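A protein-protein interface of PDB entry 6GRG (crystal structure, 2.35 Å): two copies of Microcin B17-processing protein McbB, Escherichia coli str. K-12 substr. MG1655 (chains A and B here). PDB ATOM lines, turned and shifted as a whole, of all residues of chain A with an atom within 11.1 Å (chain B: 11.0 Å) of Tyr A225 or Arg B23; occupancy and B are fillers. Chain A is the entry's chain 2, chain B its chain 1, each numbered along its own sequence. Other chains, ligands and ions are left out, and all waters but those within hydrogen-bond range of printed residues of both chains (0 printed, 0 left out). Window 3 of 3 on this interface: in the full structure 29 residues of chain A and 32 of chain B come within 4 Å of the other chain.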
ATOM      1  N   TYR A 148     -25.038  -5.134 -39.577  1.00  0.00           N
ATOM      2  CA  TYR A 148     -25.551  -6.456 -39.942  1.00  0.00           C
ATOM      3  C   TYR A 148     -26.369  -7.066 -38.797  1.00  0.00           C
ATOM      4  O   TYR A 148     -25.899  -7.136 -37.653  1.00  0.00           O
ATOM      5  CB  TYR A 148     -24.433  -7.454 -40.246  1.00  0.00           C
ATOM      6  CG  TYR A 148     -24.979  -8.837 -40.473  1.00  0.00           C
ATOM      7  CD1 TYR A 148     -25.608  -9.168 -41.659  1.00  0.00           C
ATOM      8  CD2 TYR A 148     -24.957  -9.776 -39.470  1.00  0.00           C
ATOM      9  CE1 TYR A 148     -26.152 -10.419 -41.858  1.00  0.00           C
ATOM     10  CE2 TYR A 148     -25.501 -11.037 -39.653  1.00  0.00           C
ATOM     11  CZ  TYR A 148     -26.097 -11.364 -40.851  1.00  0.00           C
ATOM     12  OH  TYR A 148     -26.637 -12.601 -41.015  1.00  0.00           O
ATOM     13  N   HIS A 149     -27.584  -7.504 -39.135  1.00  0.00           N
ATOM     14  CA  HIS A 149     -28.411  -8.371 -38.288  1.00  0.00           C
ATOM     15  C   HIS A 149     -29.186  -9.304 -39.212  1.00  0.00           C
ATOM     16  O   HIS A 149     -29.736  -8.857 -40.221  1.00  0.00           O
ATOM     17  CB  HIS A 149     -29.360  -7.590 -37.366  1.00  0.00           C
ATOM     18  CG  HIS A 149     -29.912  -8.458 -36.281  1.00  0.00           C
ATOM     19  ND1 HIS A 149     -30.419  -9.713 -36.536  1.00  0.00           N
ATOM     20  CD2 HIS A 149     -29.990  -8.295 -34.943  1.00  0.00           C
ATOM     21  CE1 HIS A 149     -30.792 -10.281 -35.402  1.00  0.00           C
ATOM     22  NE2 HIS A 149     -30.552  -9.427 -34.418  1.00  0.00           N
ATOM     23  N   ASP A 151     -31.952 -10.852 -39.042  1.00  0.00           N
ATOM     24  CA  ASP A 151     -33.388 -10.658 -39.168  1.00  0.00           C
ATOM     25  C   ASP A 151     -33.697  -9.581 -40.217  1.00  0.00           C
ATOM     26  O   ASP A 151     -34.827  -9.480 -40.686  1.00  0.00           O
ATOM     27  CB  ASP A 151     -34.016 -10.311 -37.814  1.00  0.00           C
ATOM     28  CG  ASP A 151     -34.036 -11.475 -36.830  1.00  0.00           C
ATOM     29  OD1 ASP A 151     -33.644 -12.615 -37.229  1.00  0.00           O
ATOM     30  OD2 ASP A 151     -34.392 -11.231 -35.662  1.00  0.00           O
ATOM     31  N   ALA A 216     -18.342 -16.932 -33.462  1.00  0.00           N
ATOM     32  CA  ALA A 216     -19.765 -17.291 -33.193  1.00  0.00           C
ATOM     33  C   ALA A 216     -20.240 -16.705 -31.845  1.00  0.00           C
ATOM     34  O   ALA A 216     -21.368 -16.220 -31.780  1.00  0.00           O
ATOM     35  CB  ALA A 216     -19.981 -18.793 -33.239  1.00  0.00           C
ATOM     36  N   ASN A 217     -19.389 -16.729 -30.797  1.00  0.00           N
ATOM     37  CA  ASN A 217     -19.736 -16.178 -29.467  1.00  0.00           C
ATOM     38  C   ASN A 217     -20.155 -14.701 -29.569  1.00  0.00           C
ATOM     39  O   ASN A 217     -21.149 -14.283 -28.943  1.00  0.00           O
ATOM     40  CB  ASN A 217     -18.603 -16.303 -28.442  1.00  0.00           C
ATOM     41  CG  ASN A 217     -18.276 -17.737 -28.092  1.00  0.00           C
ATOM     42  OD1 ASN A 217     -19.093 -18.634 -28.287  1.00  0.00           O
ATOM     43  ND2 ASN A 217     -17.068 -17.969 -27.603  1.00  0.00           N
ATOM     44  N   LEU A 218     -19.413 -13.903 -30.349  1.00  0.00           N
ATOM     45  CA  LEU A 218     -19.811 -12.537 -30.558  1.00  0.00           C
ATOM     46  C   LEU A 218     -21.158 -12.506 -31.296  1.00  0.00           C
ATOM     47  O   LEU A 218     -22.073 -11.790 -30.886  1.00  0.00           O
ATOM     48  CB  LEU A 218     -18.743 -11.788 -31.350  1.00  0.00           C
ATOM     49  CG  LEU A 218     -19.206 -10.410 -31.813  1.00  0.00           C
ATOM     50  CD1 LEU A 218     -19.627  -9.552 -30.620  1.00  0.00           C
ATOM     51  CD2 LEU A 218     -18.148  -9.724 -32.646  1.00  0.00           C
ATOM     52  N   LEU A 219     -21.276 -13.281 -32.378  1.00  0.00           N
ATOM     53  CA  LEU A 219     -22.471 -13.252 -33.235  1.00  0.00           C
ATOM     54  C   LEU A 219     -23.720 -13.669 -32.445  1.00  0.00           C
ATOM     55  O   LEU A 219     -24.768 -13.025 -32.538  1.00  0.00           O
ATOM     56  CB  LEU A 219     -22.258 -14.195 -34.420  1.00  0.00           C
ATOM     57  CG  LEU A 219     -21.385 -13.661 -35.545  1.00  0.00           C
ATOM     58  CD1 LEU A 219     -21.499 -14.568 -36.761  1.00  0.00           C
ATOM     59  CD2 LEU A 219     -21.766 -12.229 -35.909  1.00  0.00           C
ATOM     60  N   GLN A 220     -23.591 -14.737 -31.648  1.00  0.00           N
ATOM     61  CA  GLN A 220     -24.711 -15.254 -30.870  1.00  0.00           C
ATOM     62  C   GLN A 220     -25.047 -14.273 -29.729  1.00  0.00           C
ATOM     63  O   GLN A 220     -26.217 -14.057 -29.419  1.00  0.00           O
ATOM     64  CB  GLN A 220     -24.450 -16.683 -30.369  1.00  0.00           C
ATOM     65  CG  GLN A 220     -24.060 -17.707 -31.444  1.00  0.00           C
ATOM     66  CD  GLN A 220     -25.097 -18.070 -32.488  1.00  0.00           C
ATOM     67  OE1 GLN A 220     -25.631 -17.227 -33.207  1.00  0.00           O
ATOM     68  NE2 GLN A 220     -25.323 -19.364 -32.645  1.00  0.00           N
ATOM     69  N   LEU A 221     -24.041 -13.643 -29.116  1.00  0.00           N
ATOM     70  CA  LEU A 221     -24.325 -12.703 -28.024  1.00  0.00           C
ATOM     71  C   LEU A 221     -25.015 -11.427 -28.543  1.00  0.00           C
ATOM     72  O   LEU A 221     -25.699 -10.781 -27.792  1.00  0.00           O
ATOM     73  CB  LEU A 221     -23.035 -12.371 -27.271  1.00  0.00           C
ATOM     74  CG  LEU A 221     -23.245 -11.653 -25.942  1.00  0.00           C
ATOM     75  CD1 LEU A 221     -23.928 -12.560 -24.918  1.00  0.00           C
ATOM     76  CD2 LEU A 221     -21.930 -11.124 -25.402  1.00  0.00           C
ATOM     77  N   LEU A 222     -24.832 -11.071 -29.820  1.00  0.00           N
ATOM     78  CA  LEU A 222     -25.448  -9.870 -30.400  1.00  0.00           C
ATOM     79  C   LEU A 222     -26.939 -10.130 -30.653  1.00  0.00           C
ATOM     80  O   LEU A 222     -27.735  -9.241 -30.502  1.00  0.00           O
ATOM     81  CB  LEU A 222     -24.741  -9.488 -31.709  1.00  0.00           C
ATOM     82  CG  LEU A 222     -23.319  -8.922 -31.617  1.00  0.00           C
ATOM     83  CD1 LEU A 222     -22.719  -8.787 -33.013  1.00  0.00           C
ATOM     84  CD2 LEU A 222     -23.274  -7.574 -30.898  1.00  0.00           C
ATOM     85  N   LYS A 223     -27.300 -11.338 -31.098  1.00  0.00           N
ATOM     86  CA  LYS A 223     -28.709 -11.753 -31.089  1.00  0.00           C
ATOM     87  C   LYS A 223     -29.282 -11.564 -29.682  1.00  0.00           C
ATOM     88  O   LYS A 223     -30.138 -10.708 -29.490  1.00  0.00           O
ATOM     89  CB  LYS A 223     -28.883 -13.220 -31.484  1.00  0.00           C
ATOM     90  CG  LYS A 223     -28.662 -13.507 -32.952  1.00  0.00           C
ATOM     91  CD  LYS A 223     -29.836 -14.217 -33.583  1.00  0.00           C
ATOM     92  CE  LYS A 223     -29.793 -14.139 -35.094  1.00  0.00           C
ATOM     93  NZ  LYS A 223     -28.486 -14.606 -35.616  1.00  0.00           N
ATOM     94  N   LYS A 224     -28.741 -12.324 -28.713  1.00  0.00           N
ATOM     95  CA  LYS A 224     -29.223 -12.370 -27.328  1.00  0.00           C
ATOM     96  C   LYS A 224     -29.457 -10.949 -26.794  1.00  0.00           C
ATOM     97  O   LYS A 224     -30.415 -10.741 -26.059  1.00  0.00           O
ATOM     98  CB  LYS A 224     -28.255 -13.126 -26.413  1.00  0.00           C
ATOM     99  N   TYR A 225     -28.601  -9.986 -27.164  1.00  0.00           N
ATOM    100  CA  TYR A 225     -28.693  -8.608 -26.662  1.00  0.00           C
ATOM    101  C   TYR A 225     -29.411  -7.680 -27.661  1.00  0.00           C
ATOM    102  O   TYR A 225     -29.510  -6.460 -27.414  1.00  0.00           O
ATOM    103  CB  TYR A 225     -27.302  -8.054 -26.340  1.00  0.00           C
ATOM    104  CG  TYR A 225     -26.608  -8.574 -25.101  1.00  0.00           C
ATOM    105  CD1 TYR A 225     -27.289  -9.208 -24.069  1.00  0.00           C
ATOM    106  CD2 TYR A 225     -25.243  -8.368 -24.937  1.00  0.00           C
ATOM    107  CE1 TYR A 225     -26.631  -9.650 -22.929  1.00  0.00           C
ATOM    108  CE2 TYR A 225     -24.572  -8.800 -23.805  1.00  0.00           C
ATOM    109  CZ  TYR A 225     -25.267  -9.444 -22.798  1.00  0.00           C
ATOM    110  OH  TYR A 225     -24.601  -9.860 -21.685  1.00  0.00           O
ATOM    111  N   GLN A 226     -29.925  -8.233 -28.771  1.00  0.00           N
ATOM    112  CA  GLN A 226     -30.670  -7.454 -29.783  1.00  0.00           C
ATOM    113  C   GLN A 226     -29.802  -6.300 -30.329  1.00  0.00           C
ATOM    114  O   GLN A 226     -30.255  -5.145 -30.405  1.00  0.00           O
ATOM    115  CB  GLN A 226     -31.953  -6.874 -29.176  1.00  0.00           C
ATOM    116  CG  GLN A 226     -33.025  -7.902 -28.840  1.00  0.00           C
ATOM    117  CD  GLN A 226     -34.132  -7.291 -28.007  1.00  0.00           C
ATOM    118  OE1 GLN A 226     -34.698  -7.948 -27.138  1.00  0.00           O
ATOM    119  NE2 GLN A 226     -34.441  -6.017 -28.239  1.00  0.00           N
ATOM    120  N   MET A 227     -28.545  -6.602 -30.674  1.00  0.00           N
ATOM    121  CA  MET A 227     -27.600  -5.618 -31.207  1.00  0.00           C
ATOM    122  C   MET A 227     -27.120  -6.067 -32.596  1.00  0.00           C
ATOM    123  O   MET A 227     -26.929  -7.270 -32.835  1.00  0.00           O
ATOM    124  CB  MET A 227     -26.383  -5.482 -30.294  1.00  0.00           C
ATOM    125  CG  MET A 227     -26.698  -4.878 -28.966  1.00  0.00           C
ATOM    126  SD  MET A 227     -25.373  -5.245 -27.813  1.00  0.00           S
ATOM    127  CE  MET A 227     -24.249  -3.909 -28.185  1.00  0.00           C
ATOM    128  N   THR A 228     -26.918  -5.090 -33.491  1.00  0.00           N
ATOM    129  CA  THR A 228     -26.321  -5.312 -34.815  1.00  0.00           C
ATOM    130  C   THR A 228     -24.790  -5.472 -34.720  1.00  0.00           C
ATOM    131  O   THR A 228     -24.138  -5.116 -33.714  1.00  0.00           O
ATOM    132  CB  THR A 228     -26.720  -4.207 -35.795  1.00  0.00           C
ATOM    133  OG1 THR A 228     -26.536  -2.918 -35.213  1.00  0.00           O
ATOM    134  CG2 THR A 228     -28.161  -4.352 -36.219  1.00  0.00           C
ATOM    135  N   LEU A 229     -24.229  -6.090 -35.758  1.00  0.00           N
ATOM    136  CA  LEU A 229     -22.789  -6.166 -35.917  1.00  0.00           C
ATOM    137  C   LEU A 229     -22.368  -4.943 -36.718  1.00  0.00           C
ATOM    138  O   LEU A 229     -22.784  -4.802 -37.864  1.00  0.00           O
ATOM    139  CB  LEU A 229     -22.418  -7.461 -36.639  1.00  0.00           C
ATOM    140  CG  LEU A 229     -20.935  -7.623 -36.973  1.00  0.00           C
ATOM    141  CD1 LEU A 229     -20.099  -7.821 -35.713  1.00  0.00           C
ATOM    142  CD2 LEU A 229     -20.721  -8.778 -37.948  1.00  0.00           C
ATOM    143  N   PRO A 230     -21.603  -3.996 -36.129  1.00  0.00           N
ATOM    144  CA  PRO A 230     -21.138  -2.826 -36.874  1.00  0.00           C
ATOM    145  C   PRO A 230     -19.910  -3.158 -37.740  1.00  0.00           C
ATOM    146  O   PRO A 230     -19.085  -4.032 -37.406  1.00  0.00           O
ATOM    147  CB  PRO A 230     -20.806  -1.838 -35.746  1.00  0.00           C
ATOM    148  CG  PRO A 230     -20.341  -2.724 -34.586  1.00  0.00           C
ATOM    149  CD  PRO A 230     -21.148  -4.003 -34.720  1.00  0.00           C
ATOM    150  N   ILE B  20     -17.194   0.235 -29.932  1.00  0.00           N
ATOM    151  CA  ILE B  20     -17.630   0.023 -28.571  1.00  0.00           C
ATOM    152  C   ILE B  20     -19.134   0.313 -28.583  1.00  0.00           C
ATOM    153  O   ILE B  20     -19.527   1.459 -28.770  1.00  0.00           O
ATOM    154  CB  ILE B  20     -16.824   0.931 -27.608  1.00  0.00           C
ATOM    155  CG1 ILE B  20     -17.292   0.837 -26.156  1.00  0.00           C
ATOM    156  CG2 ILE B  20     -16.793   2.384 -28.066  1.00  0.00           C
ATOM    157  CD1 ILE B  20     -17.054  -0.516 -25.534  1.00  0.00           C
ATOM    158  N   ILE B  21     -19.961  -0.733 -28.448  1.00  0.00           N
ATOM    159  CA  ILE B  21     -21.421  -0.632 -28.656  1.00  0.00           C
ATOM    160  C   ILE B  21     -22.143  -0.976 -27.349  1.00  0.00           C
ATOM    161  O   ILE B  21     -21.713  -1.848 -26.606  1.00  0.00           O
ATOM    162  CB  ILE B  21     -21.866  -1.501 -29.855  1.00  0.00           C
ATOM    163  CG1 ILE B  21     -21.418  -2.959 -29.724  1.00  0.00           C
ATOM    164  CG2 ILE B  21     -21.346  -0.896 -31.158  1.00  0.00           C
ATOM    165  CD1 ILE B  21     -21.983  -3.890 -30.785  1.00  0.00           C
ATOM    166  N   SER B  22     -23.220  -0.238 -27.065  1.00  0.00           N
ATOM    167  CA  SER B  22     -24.043  -0.404 -25.864  1.00  0.00           C
ATOM    168  C   SER B  22     -25.523  -0.467 -26.265  1.00  0.00           C
ATOM    169  O   SER B  22     -25.933   0.250 -27.169  1.00  0.00           O
ATOM    170  CB  SER B  22     -23.811   0.730 -24.894  1.00  0.00           C
ATOM    171  OG  SER B  22     -22.496   0.694 -24.364  1.00  0.00           O
ATOM    172  N   ARG B  23     -26.301  -1.340 -25.610  1.00  0.00           N
ATOM    173  CA  ARG B  23     -27.769  -1.319 -25.673  1.00  0.00           C
ATOM    174  C   ARG B  23     -28.313  -1.992 -24.414  1.00  0.00           C
ATOM    175  O   ARG B  23     -27.813  -3.039 -23.992  1.00  0.00           O
ATOM    176  CB  ARG B  23     -28.327  -1.981 -26.939  1.00  0.00           C
ATOM    177  CG  ARG B  23     -29.685  -1.429 -27.372  1.00  0.00           C
ATOM    178  CD  ARG B  23     -30.443  -2.278 -28.383  1.00  0.00           C
ATOM    179  NE  ARG B  23     -30.975  -3.486 -27.771  1.00  0.00           N
ATOM    180  CZ  ARG B  23     -32.100  -3.542 -27.071  1.00  0.00           C
ATOM    181  NH1 ARG B  23     -32.994  -2.573 -27.168  1.00  0.00           N
ATOM    182  NH2 ARG B  23     -32.313  -4.559 -26.256  1.00  0.00           N
ATOM    183  N   ASN B  24     -29.342  -1.365 -23.833  1.00  0.00           N
ATOM    184  CA  ASN B  24     -29.707  -1.563 -22.443  1.00  0.00           C
ATOM    185  C   ASN B  24     -28.406  -1.487 -21.626  1.00  0.00           C
ATOM    186  O   ASN B  24     -27.655  -0.491 -21.739  1.00  0.00           O
ATOM    187  CB  ASN B  24     -30.516  -2.853 -22.249  1.00  0.00           C
ATOM    188  N   THR B  25     -28.118  -2.563 -20.878  1.00  0.00           N
ATOM    189  CA  THR B  25     -27.011  -2.637 -19.917  1.00  0.00           C
ATOM    190  C   THR B  25     -25.842  -3.487 -20.444  1.00  0.00           C
ATOM    191  O   THR B  25     -24.920  -3.826 -19.692  1.00  0.00           O
ATOM    192  CB  THR B  25     -27.525  -3.255 -18.619  1.00  0.00           C
ATOM    193  OG1 THR B  25     -28.100  -4.475 -19.093  1.00  0.00           O
ATOM    194  CG2 THR B  25     -28.513  -2.368 -17.891  1.00  0.00           C
ATOM    195  N   LYS B  26     -25.891  -3.846 -21.728  1.00  0.00           N
ATOM    196  CA  LYS B  26     -24.870  -4.641 -22.340  1.00  0.00           C
ATOM    197  C   LYS B  26     -23.958  -3.708 -23.152  1.00  0.00           C
ATOM    198  O   LYS B  26     -24.455  -2.868 -23.902  1.00  0.00           O
ATOM    199  CB  LYS B  26     -25.546  -5.729 -23.176  1.00  0.00           C
ATOM    200  N   THR B  27     -22.634  -3.840 -22.968  1.00  0.00           N
ATOM    201  CA  THR B  27     -21.614  -3.064 -23.727  1.00  0.00           C
ATOM    202  C   THR B  27     -20.548  -4.004 -24.300  1.00  0.00           C
ATOM    203  O   THR B  27     -19.944  -4.813 -23.589  1.00  0.00           O
ATOM    204  CB  THR B  27     -20.944  -1.983 -22.868  1.00  0.00           C
ATOM    205  OG1 THR B  27     -21.959  -1.129 -22.334  1.00  0.00           O
ATOM    206  CG2 THR B  27     -19.971  -1.139 -23.652  1.00  0.00           C
ATOM    207  N   LEU B  28     -20.320  -3.891 -25.606  1.00  0.00           N
ATOM    208  CA  LEU B  28     -19.360  -4.757 -26.288  1.00  0.00           C
ATOM    209  C   LEU B  28     -18.301  -3.924 -27.013  1.00  0.00           C
ATOM    210  O   LEU B  28     -18.622  -2.948 -27.714  1.00  0.00           O
ATOM    211  CB  LEU B  28     -20.105  -5.660 -27.270  1.00  0.00           C
ATOM    212  CG  LEU B  28     -20.897  -6.792 -26.623  1.00  0.00           C
ATOM    213  CD1 LEU B  28     -21.978  -7.305 -27.559  1.00  0.00           C
ATOM    214  CD2 LEU B  28     -19.970  -7.913 -26.228  1.00  0.00           C
ATOM    215  N   LEU B  29     -17.048  -4.363 -26.828  1.00  0.00           N
ATOM    216  CA  LEU B  29     -15.865  -3.948 -27.577  1.00  0.00           C
ATOM    217  C   LEU B  29     -15.552  -5.011 -28.650  1.00  0.00           C
ATOM    218  O   LEU B  29     -15.535  -6.225 -28.382  1.00  0.00           O
ATOM    219  CB  LEU B  29     -14.694  -3.784 -26.595  1.00  0.00           C
ATOM    220  CG  LEU B  29     -13.321  -3.593 -27.238  1.00  0.00           C
ATOM    221  CD1 LEU B  29     -13.140  -2.151 -27.690  1.00  0.00           C
ATOM    222  CD2 LEU B  29     -12.197  -3.998 -26.305  1.00  0.00           C
ATOM    223  N   ILE B  30     -15.323  -4.538 -29.879  1.00  0.00           N
ATOM    224  CA  ILE B  30     -14.964  -5.376 -31.005  1.00  0.00           C
ATOM    225  C   ILE B  30     -13.800  -4.729 -31.752  1.00  0.00           C
ATOM    226  O   ILE B  30     -13.878  -3.609 -32.155  1.00  0.00           O
ATOM    227  CB  ILE B  30     -16.156  -5.589 -31.946  1.00  0.00           C
ATOM    228  CG1 ILE B  30     -17.450  -5.858 -31.172  1.00  0.00           C
ATOM    229  CG2 ILE B  30     -15.828  -6.697 -32.933  1.00  0.00           C
ATOM    230  CD1 ILE B  30     -18.672  -5.901 -32.049  1.00  0.00           C
ATOM    231  N   SER B  35     -13.006  -9.525 -29.206  1.00  0.00           N
ATOM    232  CA  SER B  35     -14.249  -8.998 -28.725  1.00  0.00           C
ATOM    233  C   SER B  35     -14.379  -9.288 -27.218  1.00  0.00           C
ATOM    234  O   SER B  35     -13.994 -10.355 -26.774  1.00  0.00           O
ATOM    235  CB  SER B  35     -15.365  -9.587 -29.519  1.00  0.00           C
ATOM    236  OG  SER B  35     -16.615  -9.254 -28.954  1.00  0.00           O
ATOM    237  N   VAL B  36     -14.900  -8.312 -26.453  1.00  0.00           N
ATOM    238  CA  VAL B  36     -14.967  -8.358 -24.983  1.00  0.00           C
ATOM    239  C   VAL B  36     -16.338  -7.831 -24.548  1.00  0.00           C
ATOM    240  O   VAL B  36     -16.828  -6.851 -25.080  1.00  0.00           O
ATOM    241  CB  VAL B  36     -13.839  -7.539 -24.313  1.00  0.00           C
ATOM    242  CG1 VAL B  36     -13.811  -7.728 -22.803  1.00  0.00           C
ATOM    243  CG2 VAL B  36     -12.470  -7.851 -24.884  1.00  0.00           C
ATOM    244  N   ASP B  37     -16.932  -8.512 -23.561  1.00  0.00           N
ATOM    245  CA  ASP B  37     -18.107  -8.047 -22.823  1.00  0.00           C
ATOM    246  C   ASP B  37     -17.587  -7.162 -21.680  1.00  0.00           C
ATOM    247  O   ASP B  37     -17.068  -7.680 -20.693  1.00  0.00           O
ATOM    248  CB  ASP B  37     -18.944  -9.247 -22.354  1.00  0.00           C
ATOM    249  CG  ASP B  37     -20.365  -8.928 -21.897  1.00  0.00           C
ATOM    250  OD1 ASP B  37     -20.728  -7.740 -21.915  1.00  0.00           O
ATOM    251  OD2 ASP B  37     -21.106  -9.875 -21.521  1.00  0.00           O
ATOM    252  N   ILE B  38     -17.699  -5.835 -21.840  1.00  0.00           N
ATOM    253  CA  ILE B  38     -17.089  -4.841 -20.933  1.00  0.00           C
ATOM    254  C   ILE B  38     -17.944  -4.730 -19.666  1.00  0.00           C
ATOM    255  O   ILE B  38     -19.119  -4.335 -19.757  1.00  0.00           O
ATOM    256  CB  ILE B  38     -16.972  -3.472 -21.636  1.00  0.00           C
ATOM    257  CG1 ILE B  38     -16.107  -3.547 -22.898  1.00  0.00           C
ATOM    258  CG2 ILE B  38     -16.484  -2.401 -20.668  1.00  0.00           C
ATOM    259  CD1 ILE B  38     -14.721  -4.100 -22.666  1.00  0.00           C
ATOM    260  N   THR B  39     -17.356  -5.064 -18.510  1.00  0.00           N
ATOM    261  CA  THR B  39     -18.078  -5.096 -17.216  1.00  0.00           C
ATOM    262  C   THR B  39     -17.508  -4.049 -16.250  1.00  0.00           C
ATOM    263  O   THR B  39     -17.282  -4.344 -15.096  1.00  0.00           O
ATOM    264  CB  THR B  39     -18.014  -6.485 -16.561  1.00  0.00           C
ATOM    265  OG1 THR B  39     -16.651  -6.912 -16.542  1.00  0.00           O
ATOM    266  CG2 THR B  39     -18.863  -7.513 -17.275  1.00  0.00           C
ATOM    267  N   GLU B  41     -17.429   0.482 -16.002  1.00  0.00           N
ATOM    268  CA  GLU B  41     -17.850   1.792 -16.470  1.00  0.00           C
ATOM    269  C   GLU B  41     -16.618   2.609 -16.874  1.00  0.00           C
ATOM    270  O   GLU B  41     -16.582   3.207 -17.934  1.00  0.00           O
ATOM    271  CB  GLU B  41     -18.690   2.495 -15.391  1.00  0.00           C
ATOM    272  CG  GLU B  41     -20.169   2.121 -15.429  1.00  0.00           C
ATOM    273  CD  GLU B  41     -20.767   2.099 -16.838  1.00  0.00           C
ATOM    274  OE1 GLU B  41     -20.601   3.105 -17.584  1.00  0.00           O
ATOM    275  OE2 GLU B  41     -21.371   1.066 -17.209  1.00  0.00           O
ATOM    276  N   LYS B  44     -15.188   1.500 -20.093  1.00  0.00           N
ATOM    277  CA  LYS B  44     -16.152   1.915 -21.122  1.00  0.00           C
ATOM    278  C   LYS B  44     -15.901   3.382 -21.529  1.00  0.00           C
ATOM    279  O   LYS B  44     -15.923   3.730 -22.726  1.00  0.00           O
ATOM    280  CB  LYS B  44     -17.591   1.714 -20.628  1.00  0.00           C
ATOM    281  CG  LYS B  44     -18.664   2.093 -21.637  1.00  0.00           C
ATOM    282  CD  LYS B  44     -20.070   1.860 -21.171  1.00  0.00           C
ATOM    283  CE  LYS B  44     -21.070   2.645 -21.999  1.00  0.00           C
ATOM    284  NZ  LYS B  44     -22.466   2.360 -21.586  1.00  0.00           N
ATOM    285  N   GLU B  48     -14.672   4.931 -25.126  1.00  0.00           N
ATOM    286  CA  GLU B  48     -15.455   5.869 -25.933  1.00  0.00           C
ATOM    287  C   GLU B  48     -14.576   7.063 -26.306  1.00  0.00           C
ATOM    288  O   GLU B  48     -14.577   7.502 -27.453  1.00  0.00           O
ATOM    289  CB  GLU B  48     -16.722   6.292 -25.203  1.00  0.00           C
ATOM    290  CG  GLU B  48     -17.781   5.206 -25.226  1.00  0.00           C
ATOM    291  CD  GLU B  48     -18.812   5.270 -24.115  1.00  0.00           C
ATOM    292  OE1 GLU B  48     -18.450   5.665 -22.990  1.00  0.00           O
ATOM    293  OE2 GLU B  48     -19.974   4.919 -24.383  1.00  0.00           O
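NE of Arg B23 sits at hydrogen-bond distance from O of Gln A226, at 3.2 Å. The guanidinium group (NE) of Arg B23 lies within hydrogen-bond range of the backbone carbonyl oxygen (O) of Tyr A225. The side-chain carboxylate (OD2) of Asp B37 is in hydrogen-bond range of the side-chain hydroxyl (OH) of Tyr A225, at 3.5 Å.
Among the printed residues, merely in contact across the chains: Tyr A225 with Lys B26 (3.2 Å), Met A227 with Ile B21 (3.4 Å), Leu A218 with Ser B35 (3.5 Å), Leu A222 with Leu B28 (3.6 Å), Leu A218 with Ile B30 (3.8 Å), Thr A228 with Ile B21 (3.8 Å), Leu A221 with Leu B28 (3.9 Å), Met A227 with Arg B23 (3.9 Å), Leu A222 with Ile B21 (3.9 Å), Met A227 with Ser B22 (3.97 Å) and Met A227 with Leu B28 (3.98 Å).
Hydrophobic or aromatic side chains of chain A that line the printed part of chain B: Leu A218, Leu A221, Leu A222, Tyr A225 and Met A227. Along chain A the printed residues that touch a printed residue of chain B span positions 218 to 228. Along chain B the printed residues that touch a printed residue of chain A span positions 21 to 37. Among the printed residues, 14 pairs touch across the chains. Among the printed residues, no Asp or Glu carboxylate lies within 4 Å of a Lys or Arg side-chain nitrogen of the other chain.
No position is printed for both chains. Of the 14 pairs that touch across the chains among the printed residues, none has its exchanged pair printed and touching as well.
The backbone carbonyl oxygen (O) of Ile B21 lies within hydrogen-bond range of the backbone NH (N) of Leu B28 (2.7 Å). The side-chain hydroxyl (OG) of Ser B22 sits at hydrogen-bond distance from the side-chain amino group (NZ) of Lys B44, 3.2 Å away. The side-chain hydroxyl of Thr B27 sits at hydrogen-bond distance from the side-chain hydroxyl of Ser B22. The backbone carbonyl oxygen (O) of Leu A222 sits at hydrogen-bond distance from the backbone NH (N) of Met A227, 2.8 Å away. The backbone carbonyl oxygen (O) of Leu B29 lies close to the side-chain hydroxyl (OG) of Ser B35.
Of chain B, only Arg B23, Lys B26 and Asp B37 come within 4 Å of Tyr A225. Leu A221 touches one residue of chain B. No residue of chain B comes within 4 Å of Lys A224. Gln A226 touches just one residue of chain B: Arg B23 (3.2 Å). Met A227 touches just these residues of chain B: Ile B21, Ser B22, Arg B23 and Leu B28. Of chain A, only Met A227 comes within 4 Å of Ser B22. No residue of chain A comes within 4 Å of Thr B25. Lys B26 touches one residue of chain A. No residue of chain A comes within 4 Å of Thr B27. Of the printed residues of chain A, Ile B21 touches Leu A222, Met A227 and Thr A228. Of the printed residues of chain B, Thr A228 touches Ile B21 (3.8 Å). The nearest residue of chain A that does not touch Arg B23 is Lys A224 (6.5 Å). The nearest printed residue of chain B that does not touch Leu A218 is Leu B28 (4.5 Å).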
